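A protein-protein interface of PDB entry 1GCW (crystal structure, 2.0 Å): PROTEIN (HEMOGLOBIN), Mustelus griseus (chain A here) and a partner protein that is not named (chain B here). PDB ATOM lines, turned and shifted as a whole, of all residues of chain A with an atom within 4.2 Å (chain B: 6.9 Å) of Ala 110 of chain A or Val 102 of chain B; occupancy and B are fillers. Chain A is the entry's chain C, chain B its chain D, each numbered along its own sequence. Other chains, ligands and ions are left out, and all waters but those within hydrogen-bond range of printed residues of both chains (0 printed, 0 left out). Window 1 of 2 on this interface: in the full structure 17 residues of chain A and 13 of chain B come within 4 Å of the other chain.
A ring nitrogen (ND1) of His 121 of chain A lies within hydrogen-bond range of the guanidinium group (NH2) of Arg 30 of chain B. NH1 of Arg 30 of chain B lies within hydrogen-bond range of O of Phe 116 of chain A, at 2.8 Å. The side-chain hydroxyl (OG1) of Thr 111 of chain A is in hydrogen-bond range of the backbone carbonyl oxygen (O) of Lys 109 of chain B (3.3 Å). The backbone carbonyl oxygen (O) of Ala 110 of chain A lies close to the backbone carbonyl oxygen (O) of Ala 105 of chain B (3.3 Å).
OE2 of Glu 103 of chain B is in salt-bridge range of NE of Arg 30 of chain B. O of Tyr 106 of chain B is in hydrogen-bond range of NZ of Lys 109 of chain B (3.0 Å).
Among the printed residues, merely in contact across the chains: Ala 110 of chain A with Tyr 106 of chain B (3.2 Å), Thr 111 of chain A with Ala 105 of chain B (3.5 Å), Phe 116 of chain A with Tyr 106 of chain B (3.7 Å), Ala 110 of chain A with Val 102 of chain B (3.9 Å), Ile 106 of chain A with Val 102 of chain B (3.9 Å), Val 107 of chain A with Ala 105 of chain B (3.9 Å), Val 107 of chain A with Ile 101 of chain B (3.96 Å) and Phe 116 of chain A with Val 102 of chain B (3.997 Å).
Of the printed residues of chain B, Thr 111 of chain A touches Ala 105 (3.5 Å) and Lys 109 (3.3 Å). Of the printed residues of chain B, His 121 of chain A touches Arg 30 (3.0 Å). Leu 104 of chain B touches none of the printed residues of chain A. Printed residues of chain A within 4 Å of Tyr 106 of chain B: Ala 110 and Phe 116. Arg 108 of chain B touches none of the printed residues of chain A. The nearest printed residue of chain A that does not touch Ile 101 of chain B is Ala 110 of chain A (6.1 Å).
Hydrophobic or aromatic side chains of chain A within 4 Å of the printed part of chain B: Ile 106, Val 107, Ala 110, Phe 116 and His 121. Hydrophobic or aromatic side chains of chain B within 4 Å of the printed part of chain A: Ile 101, Val 102, Ala 105 and Tyr 106. Among the printed residues, 12 pairs touch across the chains.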
ATOM      1  N   ILE A 106     -12.022 -23.687  10.184  1.00  0.00           N
ATOM      2  CA  ILE A 106     -12.105 -24.122   8.794  1.00  0.00           C
ATOM      3  C   ILE A 106     -13.037 -23.211   8.005  1.00  0.00           C
ATOM      4  O   ILE A 106     -12.704 -22.790   6.899  1.00  0.00           O
ATOM      5  CB  ILE A 106     -12.630 -25.566   8.703  1.00  0.00           C
ATOM      6  CG1 ILE A 106     -11.553 -26.534   9.200  1.00  0.00           C
ATOM      7  CG2 ILE A 106     -13.094 -25.874   7.283  1.00  0.00           C
ATOM      8  CD1 ILE A 106     -10.689 -27.133   8.116  1.00  0.00           C
ATOM      9  N   VAL A 107     -14.202 -22.907   8.577  1.00  0.00           N
ATOM     10  CA  VAL A 107     -15.185 -22.045   7.921  1.00  0.00           C
ATOM     11  C   VAL A 107     -14.643 -20.636   7.725  1.00  0.00           C
ATOM     12  O   VAL A 107     -14.913 -19.986   6.708  1.00  0.00           O
ATOM     13  CB  VAL A 107     -16.489 -21.946   8.740  1.00  0.00           C
ATOM     14  CG1 VAL A 107     -17.390 -20.863   8.156  1.00  0.00           C
ATOM     15  CG2 VAL A 107     -17.212 -23.285   8.732  1.00  0.00           C
ATOM     16  N   THR A 108     -13.887 -20.164   8.711  1.00  0.00           N
ATOM     17  CA  THR A 108     -13.289 -18.840   8.652  1.00  0.00           C
ATOM     18  C   THR A 108     -12.316 -18.781   7.473  1.00  0.00           C
ATOM     19  O   THR A 108     -12.304 -17.811   6.719  1.00  0.00           O
ATOM     20  CB  THR A 108     -12.540 -18.515   9.967  1.00  0.00           C
ATOM     21  OG1 THR A 108     -13.486 -18.409  11.040  1.00  0.00           O
ATOM     22  CG2 THR A 108     -11.781 -17.204   9.843  1.00  0.00           C
ATOM     23  N   LEU A 109     -11.510 -19.825   7.310  1.00  0.00           N
ATOM     24  CA  LEU A 109     -10.560 -19.864   6.208  1.00  0.00           C
ATOM     25  C   LEU A 109     -11.269 -19.912   4.860  1.00  0.00           C
ATOM     26  O   LEU A 109     -10.809 -19.320   3.890  1.00  0.00           O
ATOM     27  CB  LEU A 109      -9.637 -21.067   6.348  1.00  0.00           C
ATOM     28  CG  LEU A 109      -8.724 -20.964   7.568  1.00  0.00           C
ATOM     29  CD1 LEU A 109      -7.950 -22.254   7.736  1.00  0.00           C
ATOM     30  CD2 LEU A 109      -7.778 -19.784   7.407  1.00  0.00           C
ATOM     31  N   ALA A 110     -12.392 -20.613   4.794  1.00  0.00           N
ATOM     32  CA  ALA A 110     -13.132 -20.713   3.545  1.00  0.00           C
ATOM     33  C   ALA A 110     -13.706 -19.349   3.158  1.00  0.00           C
ATOM     34  O   ALA A 110     -14.163 -19.137   2.031  1.00  0.00           O
ATOM     35  CB  ALA A 110     -14.250 -21.737   3.688  1.00  0.00           C
ATOM     36  N   THR A 111     -13.654 -18.420   4.103  1.00  0.00           N
ATOM     37  CA  THR A 111     -14.177 -17.078   3.902  1.00  0.00           C
ATOM     38  C   THR A 111     -13.126 -16.058   3.434  1.00  0.00           C
ATOM     39  O   THR A 111     -13.445 -15.143   2.677  1.00  0.00           O
ATOM     40  CB  THR A 111     -14.846 -16.589   5.211  1.00  0.00           C
ATOM     41  OG1 THR A 111     -16.227 -16.977   5.207  1.00  0.00           O
ATOM     42  CG2 THR A 111     -14.734 -15.080   5.361  1.00  0.00           C
ATOM     43  N   HIS A 112     -11.880 -16.215   3.876  1.00  0.00           N
ATOM     44  CA  HIS A 112     -10.815 -15.284   3.497  1.00  0.00           C
ATOM     45  C   HIS A 112      -9.890 -15.800   2.396  1.00  0.00           C
ATOM     46  O   HIS A 112      -9.455 -15.037   1.538  1.00  0.00           O
ATOM     47  CB  HIS A 112      -9.974 -14.916   4.723  1.00  0.00           C
ATOM     48  CG  HIS A 112     -10.778 -14.370   5.858  1.00  0.00           C
ATOM     49  ND1 HIS A 112     -11.304 -13.096   5.852  1.00  0.00           N
ATOM     50  CD2 HIS A 112     -11.175 -14.935   7.022  1.00  0.00           C
ATOM     51  CE1 HIS A 112     -11.992 -12.901   6.961  1.00  0.00           C
ATOM     52  NE2 HIS A 112     -11.929 -14.001   7.689  1.00  0.00           N
ATOM     53  N   PHE A 116      -9.752 -22.566  -1.510  1.00  0.00           N
ATOM     54  CA  PHE A 116      -9.906 -23.529  -0.431  1.00  0.00           C
ATOM     55  C   PHE A 116     -10.465 -24.819  -1.027  1.00  0.00           C
ATOM     56  O   PHE A 116     -11.577 -25.242  -0.713  1.00  0.00           O
ATOM     57  CB  PHE A 116     -10.859 -22.978   0.641  1.00  0.00           C
ATOM     58  CG  PHE A 116     -10.762 -23.689   1.970  1.00  0.00           C
ATOM     59  CD1 PHE A 116      -9.536 -23.800   2.631  1.00  0.00           C
ATOM     60  CD2 PHE A 116     -11.892 -24.256   2.556  1.00  0.00           C
ATOM     61  CE1 PHE A 116      -9.442 -24.463   3.851  1.00  0.00           C
ATOM     62  CE2 PHE A 116     -11.805 -24.919   3.775  1.00  0.00           C
ATOM     63  CZ  PHE A 116     -10.573 -25.023   4.423  1.00  0.00           C
ATOM     64  N   HIS A 121      -8.335 -28.035   2.134  1.00  0.00           N
ATOM     65  CA  HIS A 121      -9.241 -28.283   3.253  1.00  0.00           C
ATOM     66  C   HIS A 121      -8.715 -29.502   4.012  1.00  0.00           C
ATOM     67  O   HIS A 121      -8.499 -29.466   5.226  1.00  0.00           O
ATOM     68  CB  HIS A 121     -10.649 -28.558   2.700  1.00  0.00           C
ATOM     69  CG  HIS A 121     -11.698 -28.762   3.750  1.00  0.00           C
ATOM     70  ND1 HIS A 121     -13.044 -28.773   3.455  1.00  0.00           N
ATOM     71  CD2 HIS A 121     -11.602 -28.989   5.081  1.00  0.00           C
ATOM     72  CE1 HIS A 121     -13.733 -29.001   4.559  1.00  0.00           C
ATOM     73  NE2 HIS A 121     -12.880 -29.135   5.560  1.00  0.00           N
ATOM     74  N   ARG B  30     -16.026 -32.840  -2.007  1.00  0.00           N
ATOM     75  CA  ARG B  30     -15.208 -32.360  -0.899  1.00  0.00           C
ATOM     76  C   ARG B  30     -15.226 -33.410   0.224  1.00  0.00           C
ATOM     77  O   ARG B  30     -14.176 -33.780   0.763  1.00  0.00           O
ATOM     78  CB  ARG B  30     -15.761 -31.028  -0.379  1.00  0.00           C
ATOM     79  CG  ARG B  30     -14.948 -30.411   0.744  1.00  0.00           C
ATOM     80  CD  ARG B  30     -15.490 -29.041   1.128  1.00  0.00           C
ATOM     81  NE  ARG B  30     -15.260 -28.063   0.071  1.00  0.00           N
ATOM     82  CZ  ARG B  30     -14.109 -27.432  -0.123  1.00  0.00           C
ATOM     83  NH1 ARG B  30     -13.993 -26.558  -1.115  1.00  0.00           N
ATOM     84  NH2 ARG B  30     -13.076 -27.675   0.677  1.00  0.00           N
ATOM     85  N   THR B  97     -23.256 -32.147   5.496  1.00  0.00           N
ATOM     86  CA  THR B  97     -23.757 -30.797   5.723  1.00  0.00           C
ATOM     87  C   THR B  97     -22.661 -29.792   6.058  1.00  0.00           C
ATOM     88  O   THR B  97     -22.743 -28.636   5.661  1.00  0.00           O
ATOM     89  CB  THR B  97     -24.824 -30.768   6.836  1.00  0.00           C
ATOM     90  OG1 THR B  97     -24.243 -31.175   8.084  1.00  0.00           O
ATOM     91  CG2 THR B  97     -25.982 -31.689   6.464  1.00  0.00           C
ATOM     92  N   ASP B  98     -21.639 -30.226   6.786  1.00  0.00           N
ATOM     93  CA  ASP B  98     -20.539 -29.332   7.135  1.00  0.00           C
ATOM     94  C   ASP B  98     -19.857 -28.868   5.849  1.00  0.00           C
ATOM     95  O   ASP B  98     -19.463 -27.708   5.716  1.00  0.00           O
ATOM     96  CB  ASP B  98     -19.527 -30.058   8.014  1.00  0.00           C
ATOM     97  CG  ASP B  98     -19.952 -30.118   9.463  1.00  0.00           C
ATOM     98  OD1 ASP B  98     -19.209 -30.711  10.270  1.00  0.00           O
ATOM     99  OD2 ASP B  98     -21.024 -29.574   9.800  1.00  0.00           O
ATOM    100  N   CYS B  99     -19.732 -29.789   4.898  1.00  0.00           N
ATOM    101  CA  CYS B  99     -19.104 -29.500   3.617  1.00  0.00           C
ATOM    102  C   CYS B  99     -19.938 -28.517   2.800  1.00  0.00           C
ATOM    103  O   CYS B  99     -19.395 -27.658   2.105  1.00  0.00           O
ATOM    104  CB  CYS B  99     -18.888 -30.798   2.837  1.00  0.00           C
ATOM    105  SG  CYS B  99     -17.539 -31.799   3.502  1.00  0.00           S
ATOM    106  N   ILE B 100     -21.256 -28.645   2.881  1.00  0.00           N
ATOM    107  CA  ILE B 100     -22.149 -27.739   2.168  1.00  0.00           C
ATOM    108  C   ILE B 100     -21.989 -26.347   2.780  1.00  0.00           C
ATOM    109  O   ILE B 100     -22.074 -25.341   2.085  1.00  0.00           O
ATOM    110  CB  ILE B 100     -23.615 -28.182   2.318  1.00  0.00           C
ATOM    111  CG1 ILE B 100     -23.848 -29.482   1.548  1.00  0.00           C
ATOM    112  CG2 ILE B 100     -24.549 -27.083   1.844  1.00  0.00           C
ATOM    113  CD1 ILE B 100     -25.227 -30.061   1.755  1.00  0.00           C
ATOM    114  N   ILE B 101     -21.755 -26.292   4.087  1.00  0.00           N
ATOM    115  CA  ILE B 101     -21.577 -25.012   4.761  1.00  0.00           C
ATOM    116  C   ILE B 101     -20.266 -24.397   4.292  1.00  0.00           C
ATOM    117  O   ILE B 101     -20.200 -23.201   4.012  1.00  0.00           O
ATOM    118  CB  ILE B 101     -21.552 -25.176   6.311  1.00  0.00           C
ATOM    119  CG1 ILE B 101     -22.956 -24.979   6.875  1.00  0.00           C
ATOM    120  CG2 ILE B 101     -20.639 -24.141   6.949  1.00  0.00           C
ATOM    121  CD1 ILE B 101     -23.161 -25.628   8.223  1.00  0.00           C
ATOM    122  N   VAL B 102     -19.221 -25.217   4.210  1.00  0.00           N
ATOM    123  CA  VAL B 102     -17.918 -24.739   3.765  1.00  0.00           C
ATOM    124  C   VAL B 102     -18.016 -24.228   2.327  1.00  0.00           C
ATOM    125  O   VAL B 102     -17.376 -23.242   1.957  1.00  0.00           O
ATOM    126  CB  VAL B 102     -16.860 -25.860   3.833  1.00  0.00           C
ATOM    127  CG1 VAL B 102     -15.671 -25.512   2.953  1.00  0.00           C
ATOM    128  CG2 VAL B 102     -16.399 -26.049   5.262  1.00  0.00           C
ATOM    129  N   GLU B 103     -18.825 -24.900   1.516  1.00  0.00           N
ATOM    130  CA  GLU B 103     -18.997 -24.499   0.125  1.00  0.00           C
ATOM    131  C   GLU B 103     -19.706 -23.147   0.057  1.00  0.00           C
ATOM    132  O   GLU B 103     -19.358 -22.288  -0.755  1.00  0.00           O
ATOM    133  CB  GLU B 103     -19.799 -25.559  -0.634  1.00  0.00           C
ATOM    134  CG  GLU B 103     -18.974 -26.759  -1.062  1.00  0.00           C
ATOM    135  CD  GLU B 103     -17.856 -26.383  -2.011  1.00  0.00           C
ATOM    136  OE1 GLU B 103     -18.079 -25.504  -2.867  1.00  0.00           O
ATOM    137  OE2 GLU B 103     -16.755 -26.960  -1.905  1.00  0.00           O
ATOM    138  N   LEU B 104     -20.705 -22.971   0.918  1.00  0.00           N
ATOM    139  CA  LEU B 104     -21.457 -21.724   0.981  1.00  0.00           C
ATOM    140  C   LEU B 104     -20.548 -20.628   1.532  1.00  0.00           C
ATOM    141  O   LEU B 104     -20.544 -19.509   1.034  1.00  0.00           O
ATOM    142  CB  LEU B 104     -22.673 -21.887   1.892  1.00  0.00           C
ATOM    143  CG  LEU B 104     -23.958 -22.418   1.260  1.00  0.00           C
ATOM    144  CD1 LEU B 104     -24.932 -22.797   2.367  1.00  0.00           C
ATOM    145  CD2 LEU B 104     -24.568 -21.368   0.341  1.00  0.00           C
ATOM    146  N   ALA B 105     -19.782 -20.964   2.564  1.00  0.00           N
ATOM    147  CA  ALA B 105     -18.864 -20.020   3.184  1.00  0.00           C
ATOM    148  C   ALA B 105     -17.865 -19.571   2.145  1.00  0.00           C
ATOM    149  O   ALA B 105     -17.364 -18.451   2.192  1.00  0.00           O
ATOM    150  CB  ALA B 105     -18.132 -20.674   4.341  1.00  0.00           C
ATOM    151  N   TYR B 106     -17.568 -20.456   1.205  1.00  0.00           N
ATOM    152  CA  TYR B 106     -16.612 -20.122   0.166  1.00  0.00           C
ATOM    153  C   TYR B 106     -17.258 -19.214  -0.866  1.00  0.00           C
ATOM    154  O   TYR B 106     -16.640 -18.278  -1.371  1.00  0.00           O
ATOM    155  CB  TYR B 106     -16.097 -21.391  -0.505  1.00  0.00           C
ATOM    156  CG  TYR B 106     -14.933 -21.137  -1.429  1.00  0.00           C
ATOM    157  CD1 TYR B 106     -15.021 -21.438  -2.787  1.00  0.00           C
ATOM    158  CD2 TYR B 106     -13.745 -20.585  -0.948  1.00  0.00           C
ATOM    159  CE1 TYR B 106     -13.962 -21.197  -3.643  1.00  0.00           C
ATOM    160  CE2 TYR B 106     -12.676 -20.340  -1.798  1.00  0.00           C
ATOM    161  CZ  TYR B 106     -12.793 -20.649  -3.145  1.00  0.00           C
ATOM    162  OH  TYR B 106     -11.742 -20.416  -4.001  1.00  0.00           O
ATOM    163  N   LEU B 107     -18.516 -19.494  -1.173  1.00  0.00           N
ATOM    164  CA  LEU B 107     -19.234 -18.697  -2.145  1.00  0.00           C
ATOM    165  C   LEU B 107     -19.379 -17.263  -1.663  1.00  0.00           C
ATOM    166  O   LEU B 107     -18.713 -16.365  -2.171  1.00  0.00           O
ATOM    167  CB  LEU B 107     -20.616 -19.298  -2.406  1.00  0.00           C
ATOM    168  CG  LEU B 107     -21.346 -18.778  -3.646  1.00  0.00           C
ATOM    169  CD1 LEU B 107     -20.452 -18.935  -4.872  1.00  0.00           C
ATOM    170  CD2 LEU B 107     -22.654 -19.536  -3.824  1.00  0.00           C
ATOM    171  N   ARG B 108     -20.238 -17.063  -0.668  1.00  0.00           N
ATOM    172  CA  ARG B 108     -20.511 -15.740  -0.108  1.00  0.00           C
ATOM    173  C   ARG B 108     -19.337 -14.983   0.529  1.00  0.00           C
ATOM    174  O   ARG B 108     -19.491 -13.823   0.897  1.00  0.00           O
ATOM    175  CB  ARG B 108     -21.655 -15.842   0.908  1.00  0.00           C
ATOM    176  CG  ARG B 108     -23.041 -15.953   0.281  1.00  0.00           C
ATOM    177  CD  ARG B 108     -23.752 -17.206   0.763  1.00  0.00           C
ATOM    178  NE  ARG B 108     -25.193 -17.171   0.523  1.00  0.00           N
ATOM    179  CZ  ARG B 108     -26.085 -16.664   1.370  1.00  0.00           C
ATOM    180  NH1 ARG B 108     -27.372 -16.682   1.059  1.00  0.00           N
ATOM    181  NH2 ARG B 108     -25.698 -16.131   2.523  1.00  0.00           N
ATOM    182  N   LYS B 109     -18.176 -15.618   0.661  1.00  0.00           N
ATOM    183  CA  LYS B 109     -17.006 -14.967   1.257  1.00  0.00           C
ATOM    184  C   LYS B 109     -17.354 -14.224   2.559  1.00  0.00           C
ATOM    185  O   LYS B 109     -18.001 -14.799   3.430  1.00  0.00           O
ATOM    186  CB  LYS B 109     -16.361 -14.010   0.246  1.00  0.00           C
ATOM    187  CG  LYS B 109     -15.635 -14.717  -0.901  1.00  0.00           C
ATOM    188  CD  LYS B 109     -14.166 -14.956  -0.573  1.00  0.00           C
ATOM    189  CE  LYS B 109     -13.460 -15.817  -1.628  1.00  0.00           C
ATOM    190  NZ  LYS B 109     -14.399 -16.633  -2.451  1.00  0.00           N
ATOM    191  N   ASP B 110     -16.946 -12.961   2.700  1.00  0.00           N
ATOM    192  CA  ASP B 110     -17.236 -12.215   3.936  1.00  0.00           C
ATOM    193  C   ASP B 110     -18.719 -11.919   4.208  1.00  0.00           C
ATOM    194  O   ASP B 110     -19.072 -11.457   5.296  1.00  0.00           O
ATOM    195  CB  ASP B 110     -16.427 -10.902   4.011  1.00  0.00           C
ATOM    196  CG  ASP B 110     -16.106 -10.312   2.644  1.00  0.00           C
ATOM    197  OD1 ASP B 110     -14.915 -10.339   2.255  1.00  0.00           O
ATOM    198  OD2 ASP B 110     -17.036  -9.812   1.968  1.00  0.00           O
ATOM    199  N   PHE B 112     -20.694 -14.034   4.636  1.00  0.00           N
ATOM    200  CA  PHE B 112     -21.065 -15.211   5.428  1.00  0.00           C
ATOM    201  C   PHE B 112     -20.616 -15.009   6.880  1.00  0.00           C
ATOM    202  O   PHE B 112     -19.746 -15.721   7.387  1.00  0.00           O
ATOM    203  CB  PHE B 112     -20.402 -16.469   4.842  1.00  0.00           C
ATOM    204  CG  PHE B 112     -21.094 -17.755   5.212  1.00  0.00           C
ATOM    205  CD1 PHE B 112     -22.266 -18.144   4.565  1.00  0.00           C
ATOM    206  CD2 PHE B 112     -20.572 -18.581   6.213  1.00  0.00           C
ATOM    207  CE1 PHE B 112     -22.917 -19.341   4.907  1.00  0.00           C
ATOM    208  CE2 PHE B 112     -21.213 -19.780   6.566  1.00  0.00           C
ATOM    209  CZ  PHE B 112     -22.387 -20.159   5.909  1.00  0.00           C
